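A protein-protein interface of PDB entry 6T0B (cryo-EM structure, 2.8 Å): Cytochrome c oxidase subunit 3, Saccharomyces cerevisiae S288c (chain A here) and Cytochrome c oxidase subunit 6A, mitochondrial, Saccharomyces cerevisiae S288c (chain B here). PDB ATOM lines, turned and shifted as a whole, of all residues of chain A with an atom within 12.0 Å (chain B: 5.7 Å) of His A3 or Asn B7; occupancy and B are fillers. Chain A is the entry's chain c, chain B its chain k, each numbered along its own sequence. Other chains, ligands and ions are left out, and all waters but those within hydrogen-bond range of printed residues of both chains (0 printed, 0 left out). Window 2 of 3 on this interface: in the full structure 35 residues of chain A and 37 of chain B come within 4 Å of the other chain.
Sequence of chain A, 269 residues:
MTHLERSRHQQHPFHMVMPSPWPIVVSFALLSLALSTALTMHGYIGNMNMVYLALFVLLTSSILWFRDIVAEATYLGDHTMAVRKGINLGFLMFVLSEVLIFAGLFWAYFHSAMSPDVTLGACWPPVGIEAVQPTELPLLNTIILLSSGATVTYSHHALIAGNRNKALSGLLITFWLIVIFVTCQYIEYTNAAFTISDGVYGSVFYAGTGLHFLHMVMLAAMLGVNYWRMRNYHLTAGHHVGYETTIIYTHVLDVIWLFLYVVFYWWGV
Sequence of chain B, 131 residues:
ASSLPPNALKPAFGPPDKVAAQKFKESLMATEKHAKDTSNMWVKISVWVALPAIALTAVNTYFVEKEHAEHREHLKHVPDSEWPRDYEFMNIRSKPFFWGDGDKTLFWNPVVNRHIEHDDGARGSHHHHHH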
ATOM      1  N   MET A   1     -13.132 -19.602 -30.673  1.00  0.00           N
ATOM      2  CA  MET A   1     -12.756 -18.616 -29.670  1.00  0.00           C
ATOM      3  C   MET A   1     -13.825 -17.525 -29.554  1.00  0.00           C
ATOM      4  O   MET A   1     -14.604 -17.310 -30.480  1.00  0.00           O
ATOM      5  CB  MET A   1     -11.382 -18.016 -30.007  1.00  0.00           C
ATOM      6  CG  MET A   1     -11.362 -17.115 -31.225  1.00  0.00           C
ATOM      7  SD  MET A   1      -9.881 -16.149 -31.487  1.00  0.00           S
ATOM      8  CE  MET A   1      -9.047 -16.964 -32.695  1.00  0.00           C
ATOM      9  N   THR A   2     -13.875 -16.854 -28.406  1.00  0.00           N
ATOM     10  CA  THR A   2     -14.937 -15.898 -28.151  1.00  0.00           C
ATOM     11  C   THR A   2     -14.678 -14.591 -28.886  1.00  0.00           C
ATOM     12  O   THR A   2     -13.596 -14.350 -29.415  1.00  0.00           O
ATOM     13  CB  THR A   2     -15.080 -15.623 -26.661  1.00  0.00           C
ATOM     14  OG1 THR A   2     -14.023 -14.767 -26.231  1.00  0.00           O
ATOM     15  CG2 THR A   2     -15.021 -16.905 -25.888  1.00  0.00           C
ATOM     16  N   HIS A   3     -15.708 -13.745 -28.910  1.00  0.00           N
ATOM     17  CA  HIS A   3     -15.597 -12.434 -29.535  1.00  0.00           C
ATOM     18  C   HIS A   3     -14.627 -11.543 -28.775  1.00  0.00           C
ATOM     19  O   HIS A   3     -13.865 -10.778 -29.386  1.00  0.00           O
ATOM     20  CB  HIS A   3     -16.974 -11.781 -29.592  1.00  0.00           C
ATOM     21  CG  HIS A   3     -17.807 -12.218 -30.753  1.00  0.00           C
ATOM     22  ND1 HIS A   3     -17.348 -12.188 -32.050  1.00  0.00           N
ATOM     23  CD2 HIS A   3     -19.075 -12.680 -30.815  1.00  0.00           C
ATOM     24  CE1 HIS A   3     -18.299 -12.610 -32.861  1.00  0.00           C
ATOM     25  NE2 HIS A   3     -19.357 -12.918 -32.137  1.00  0.00           N
ATOM     26  N   LEU A   4     -14.634 -11.657 -27.445  1.00  0.00           N
ATOM     27  CA  LEU A   4     -13.783 -10.842 -26.589  1.00  0.00           C
ATOM     28  C   LEU A   4     -12.314 -11.118 -26.846  1.00  0.00           C
ATOM     29  O   LEU A   4     -11.481 -10.208 -26.800  1.00  0.00           O
ATOM     30  CB  LEU A   4     -14.127 -11.120 -25.131  1.00  0.00           C
ATOM     31  CG  LEU A   4     -13.190 -10.599 -24.055  1.00  0.00           C
ATOM     32  CD1 LEU A   4     -13.365  -9.106 -23.890  1.00  0.00           C
ATOM     33  CD2 LEU A   4     -13.447 -11.326 -22.760  1.00  0.00           C
ATOM     34  N   GLU A   5     -11.987 -12.357 -27.161  1.00  0.00           N
ATOM     35  CA  GLU A   5     -10.605 -12.722 -27.378  1.00  0.00           C
ATOM     36  C   GLU A   5     -10.205 -12.630 -28.841  1.00  0.00           C
ATOM     37  O   GLU A   5      -9.036 -12.374 -29.134  1.00  0.00           O
ATOM     38  CB  GLU A   5     -10.370 -14.121 -26.814  1.00  0.00           C
ATOM     39  CG  GLU A   5      -8.956 -14.487 -26.699  1.00  0.00           C
ATOM     40  CD  GLU A   5      -8.489 -15.257 -27.869  1.00  0.00           C
ATOM     41  OE1 GLU A   5      -9.284 -16.067 -28.364  1.00  0.00           O
ATOM     42  OE2 GLU A   5      -7.354 -15.009 -28.336  1.00  0.00           O
ATOM     43  N   ARG A   6     -11.142 -12.834 -29.766  1.00  0.00           N
ATOM     44  CA  ARG A   6     -10.878 -12.582 -31.178  1.00  0.00           C
ATOM     45  C   ARG A   6     -10.625 -11.110 -31.435  1.00  0.00           C
ATOM     46  O   ARG A   6      -9.894 -10.760 -32.363  1.00  0.00           O
ATOM     47  CB  ARG A   6     -12.052 -13.069 -32.023  1.00  0.00           C
ATOM     48  CG  ARG A   6     -11.889 -12.958 -33.529  1.00  0.00           C
ATOM     49  CD  ARG A   6     -10.605 -13.602 -33.985  1.00  0.00           C
ATOM     50  NE  ARG A   6     -10.353 -13.479 -35.414  1.00  0.00           N
ATOM     51  CZ  ARG A   6      -9.451 -12.669 -35.943  1.00  0.00           C
ATOM     52  NH1 ARG A   6      -9.293 -12.642 -37.245  1.00  0.00           N
ATOM     53  NH2 ARG A   6      -8.711 -11.891 -35.173  1.00  0.00           N
ATOM     54  N   SER A   7     -11.186 -10.233 -30.608  1.00  0.00           N
ATOM     55  CA  SER A   7     -10.965  -8.811 -30.799  1.00  0.00           C
ATOM     56  C   SER A   7      -9.558  -8.361 -30.434  1.00  0.00           C
ATOM     57  O   SER A   7      -9.208  -7.217 -30.728  1.00  0.00           O
ATOM     58  CB  SER A   7     -11.989  -8.029 -29.988  1.00  0.00           C
ATOM     59  OG  SER A   7     -13.289  -8.513 -30.246  1.00  0.00           O
ATOM     60  N   ARG A   8      -8.741  -9.212 -29.817  1.00  0.00           N
ATOM     61  CA  ARG A   8      -7.366  -8.860 -29.494  1.00  0.00           C
ATOM     62  C   ARG A   8      -6.372  -9.288 -30.559  1.00  0.00           C
ATOM     63  O   ARG A   8      -5.210  -9.537 -30.234  1.00  0.00           O
ATOM     64  CB  ARG A   8      -6.955  -9.472 -28.162  1.00  0.00           C
ATOM     65  CG  ARG A   8      -7.945  -9.290 -27.068  1.00  0.00           C
ATOM     66  CD  ARG A   8      -7.739 -10.348 -26.020  1.00  0.00           C
ATOM     67  NE  ARG A   8      -6.537 -10.106 -25.238  1.00  0.00           N
ATOM     68  CZ  ARG A   8      -6.062 -10.950 -24.332  1.00  0.00           C
ATOM     69  NH1 ARG A   8      -6.687 -12.093 -24.100  1.00  0.00           N
ATOM     70  NH2 ARG A   8      -4.961 -10.652 -23.663  1.00  0.00           N
ATOM     71  N   HIS A   9      -6.797  -9.409 -31.810  1.00  0.00           N
ATOM     72  CA  HIS A   9      -5.911  -9.779 -32.899  1.00  0.00           C
ATOM     73  C   HIS A   9      -6.306  -8.950 -34.110  1.00  0.00           C
ATOM     74  O   HIS A   9      -7.076  -7.995 -34.001  1.00  0.00           O
ATOM     75  CB  HIS A   9      -5.965 -11.285 -33.156  1.00  0.00           C
ATOM     76  CG  HIS A   9      -5.454 -12.115 -32.020  1.00  0.00           C
ATOM     77  ND1 HIS A   9      -6.231 -12.458 -30.939  1.00  0.00           N
ATOM     78  CD2 HIS A   9      -4.248 -12.684 -31.806  1.00  0.00           C
ATOM     79  CE1 HIS A   9      -5.528 -13.202 -30.108  1.00  0.00           C
ATOM     80  NE2 HIS A   9      -4.320 -13.349 -30.608  1.00  0.00           N
ATOM     81  N   GLN A  10      -5.805  -9.314 -35.284  1.00  0.00           N
ATOM     82  CA  GLN A  10      -5.694  -8.319 -36.339  1.00  0.00           C
ATOM     83  C   GLN A  10      -6.879  -8.240 -37.291  1.00  0.00           C
ATOM     84  O   GLN A  10      -6.993  -7.232 -37.997  1.00  0.00           O
ATOM     85  CB  GLN A  10      -4.427  -8.556 -37.159  1.00  0.00           C
ATOM     86  CG  GLN A  10      -3.745  -7.268 -37.523  1.00  0.00           C
ATOM     87  CD  GLN A  10      -2.573  -7.459 -38.418  1.00  0.00           C
ATOM     88  OE1 GLN A  10      -1.973  -8.518 -38.443  1.00  0.00           O
ATOM     89  NE2 GLN A  10      -2.227  -6.431 -39.163  1.00  0.00           N
ATOM     90  N   GLN A  11      -7.718  -9.275 -37.375  1.00  0.00           N
ATOM     91  CA  GLN A  11      -8.891  -9.424 -38.250  1.00  0.00           C
ATOM     92  C   GLN A  11      -8.559  -9.537 -39.734  1.00  0.00           C
ATOM     93  O   GLN A  11      -9.472  -9.771 -40.527  1.00  0.00           O
ATOM     94  CB  GLN A  11      -9.932  -8.299 -38.105  1.00  0.00           C
ATOM     95  CG  GLN A  11     -10.588  -8.187 -36.757  1.00  0.00           C
ATOM     96  CD  GLN A  11     -11.525  -9.323 -36.487  1.00  0.00           C
ATOM     97  OE1 GLN A  11     -11.605  -9.822 -35.367  1.00  0.00           O
ATOM     98  NE2 GLN A  11     -12.241  -9.753 -37.515  1.00  0.00           N
ATOM     99  N   PRO B   5     -19.461  -5.444 -22.597  1.00  0.00           N
ATOM    100  CA  PRO B   5     -20.470  -5.703 -23.629  1.00  0.00           C
ATOM    101  C   PRO B   5     -21.234  -6.975 -23.314  1.00  0.00           C
ATOM    102  O   PRO B   5     -20.692  -7.886 -22.671  1.00  0.00           O
ATOM    103  CB  PRO B   5     -19.637  -5.854 -24.913  1.00  0.00           C
ATOM    104  CG  PRO B   5     -18.310  -5.270 -24.587  1.00  0.00           C
ATOM    105  CD  PRO B   5     -18.100  -5.558 -23.136  1.00  0.00           C
ATOM    106  N   PRO B   6     -22.506  -7.071 -23.731  1.00  0.00           N
ATOM    107  CA  PRO B   6     -23.273  -8.296 -23.466  1.00  0.00           C
ATOM    108  C   PRO B   6     -22.849  -9.448 -24.352  1.00  0.00           C
ATOM    109  O   PRO B   6     -22.812 -10.605 -23.914  1.00  0.00           O
ATOM    110  CB  PRO B   6     -24.719  -7.886 -23.766  1.00  0.00           C
ATOM    111  CG  PRO B   6     -24.702  -6.396 -23.955  1.00  0.00           C
ATOM    112  CD  PRO B   6     -23.326  -6.055 -24.410  1.00  0.00           C
ATOM    113  N   ASN B   7     -22.482  -9.118 -25.591  1.00  0.00           N
ATOM    114  CA  ASN B   7     -22.224 -10.107 -26.630  1.00  0.00           C
ATOM    115  C   ASN B   7     -20.743 -10.436 -26.797  1.00  0.00           C
ATOM    116  O   ASN B   7     -20.340 -10.888 -27.869  1.00  0.00           O
ATOM    117  CB  ASN B   7     -22.803  -9.627 -27.962  1.00  0.00           C
ATOM    118  CG  ASN B   7     -22.327  -8.254 -28.316  1.00  0.00           C
ATOM    119  OD1 ASN B   7     -22.306  -7.361 -27.456  1.00  0.00           O
ATOM    120  ND2 ASN B   7     -21.954  -8.058 -29.564  1.00  0.00           N
ATOM    121  N   ALA B   8     -19.923 -10.207 -25.774  1.00  0.00           N
ATOM    122  CA  ALA B   8     -18.496 -10.452 -25.889  1.00  0.00           C
ATOM    123  C   ALA B   8     -18.130 -11.917 -25.749  1.00  0.00           C
ATOM    124  O   ALA B   8     -17.052 -12.306 -26.200  1.00  0.00           O
ATOM    125  CB  ALA B   8     -17.752  -9.647 -24.831  1.00  0.00           C
ATOM    126  N   LEU B   9     -18.985 -12.731 -25.137  1.00  0.00           N
ATOM    127  CA  LEU B   9     -18.621 -14.085 -24.745  1.00  0.00           C
ATOM    128  C   LEU B   9     -19.238 -15.149 -25.637  1.00  0.00           C
ATOM    129  O   LEU B   9     -19.087 -16.340 -25.353  1.00  0.00           O
ATOM    130  CB  LEU B   9     -19.019 -14.342 -23.290  1.00  0.00           C
ATOM    131  CG  LEU B   9     -18.045 -13.945 -22.177  1.00  0.00           C
ATOM    132  CD1 LEU B   9     -16.721 -14.686 -22.337  1.00  0.00           C
ATOM    133  CD2 LEU B   9     -17.820 -12.442 -22.062  1.00  0.00           C
ATOM    134  N   LYS B  10     -19.898 -14.769 -26.651  1.00  0.00           N
ATOM    135  CA  LYS B  10     -20.409 -15.726 -27.618  1.00  0.00           C
ATOM    136  C   LYS B  10     -19.326 -16.124 -28.615  1.00  0.00           C
ATOM    137  O   LYS B  10     -18.417 -15.338 -28.890  1.00  0.00           O
ATOM    138  CB  LYS B  10     -21.601 -15.141 -28.365  1.00  0.00           C
ATOM    139  CG  LYS B  10     -22.855 -15.130 -27.540  1.00  0.00           C
ATOM    140  CD  LYS B  10     -24.060 -14.717 -28.373  1.00  0.00           C
ATOM    141  CE  LYS B  10     -24.070 -13.211 -28.655  1.00  0.00           C
ATOM    142  NZ  LYS B  10     -24.394 -12.461 -27.414  1.00  0.00           N
ATOM    143  N   PRO B  11     -19.387 -17.339 -29.169  1.00  0.00           N
ATOM    144  CA  PRO B  11     -18.327 -17.773 -30.086  1.00  0.00           C
ATOM    145  C   PRO B  11     -18.366 -17.027 -31.408  1.00  0.00           C
ATOM    146  O   PRO B  11     -19.433 -16.729 -31.951  1.00  0.00           O
ATOM    147  CB  PRO B  11     -18.612 -19.267 -30.284  1.00  0.00           C
ATOM    148  CG  PRO B  11     -19.448 -19.655 -29.122  1.00  0.00           C
ATOM    149  CD  PRO B  11     -20.291 -18.455 -28.843  1.00  0.00           C
ATOM    150  N   ALA B  12     -17.180 -16.734 -31.925  1.00  0.00           N
ATOM    151  CA  ALA B  12     -17.030 -15.912 -33.112  1.00  0.00           C
ATOM    152  C   ALA B  12     -17.038 -16.710 -34.404  1.00  0.00           C
ATOM    153  O   ALA B  12     -16.970 -16.108 -35.479  1.00  0.00           O
ATOM    154  CB  ALA B  12     -15.735 -15.103 -33.023  1.00  0.00           C
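The backbone carbonyl oxygen (O) of Met A1 is in hydrogen-bond range of the backbone NH (N) of Ala B12, at 3.0 Å. The backbone NH (N) of His A3 sits at hydrogen-bond distance from the backbone carbonyl oxygen (O) of Ala B8, 3.3 Å away. The backbone NH (N) of His A3 sits at hydrogen-bond distance from the backbone carbonyl oxygen (O) of Lys B10 (3.1 Å). N of Leu A4 lies within hydrogen-bond range of O of Ala B8, 2.8 Å away.
The side-chain hydroxyl of Thr A2 lies close to the backbone NH of Leu A4 (3.4 Å). OG1 of Thr A2 is in hydrogen-bond range of N of Glu A5 (3.3 Å). O of His A3 is in hydrogen-bond range of OG of Ser A7, 2.5 Å away.
Pro B11 touches Met A1. Thr A2 touches Ala B8 (CB to O, 3.9 Å). Lys B10 touches Thr A2 (O to CA, 3.6 Å). Asn B7 touches His A3. NE2 of His A3 touches O of Pro B11, at 3.8 Å. CB of Ala B12 touches ND1 of His A3, at 3.5 Å.
Printed residues of chain B within 4 Å of Met A1: Pro B11 (3.8 Å) and Ala B12 (3.0 Å). Of the printed residues of chain B, Thr A2 touches Ala B8 (3.9 Å) and Lys B10 (3.6 Å). Of chain B, only Asn B7, Ala B8, Lys B10, Pro B11 and Ala B12 come within 4 Å of His A3. Printed residues of chain B within 4 Å of Leu A4: Ala B8. No residue of chain A comes within 4 Å of Pro B5. No residue of chain A comes within 4 Å of Pro B6. Asn B7 touches just one residue of chain A: His A3 (3.7 Å). No residue of chain A comes within 4 Å of Leu B9. Lys B10 touches two residues of chain A. Of the printed residues of chain A, Pro B11 touches Met A1 and His A3. The nearest residue of chain B that does not touch His A3 is Leu B9 (5.0 Å). The nearest residue of chain A that does not touch Asn B7 is Leu A4 (5.8 Å).
Of the 11 printed residues of chain A, 4 touch a printed residue of chain B. Printed residues of chain A that touch a printed residue of chain B: Met A1, Thr A2, His A3 and Leu A4. Hydrophobic or aromatic side chains of chain A within 4 Å of the printed part of chain B: His A3 and Leu A4. Hydrophobic or aromatic side chains of chain B within 4 Å of the printed part of chain A: Ala B8 and Ala B12.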
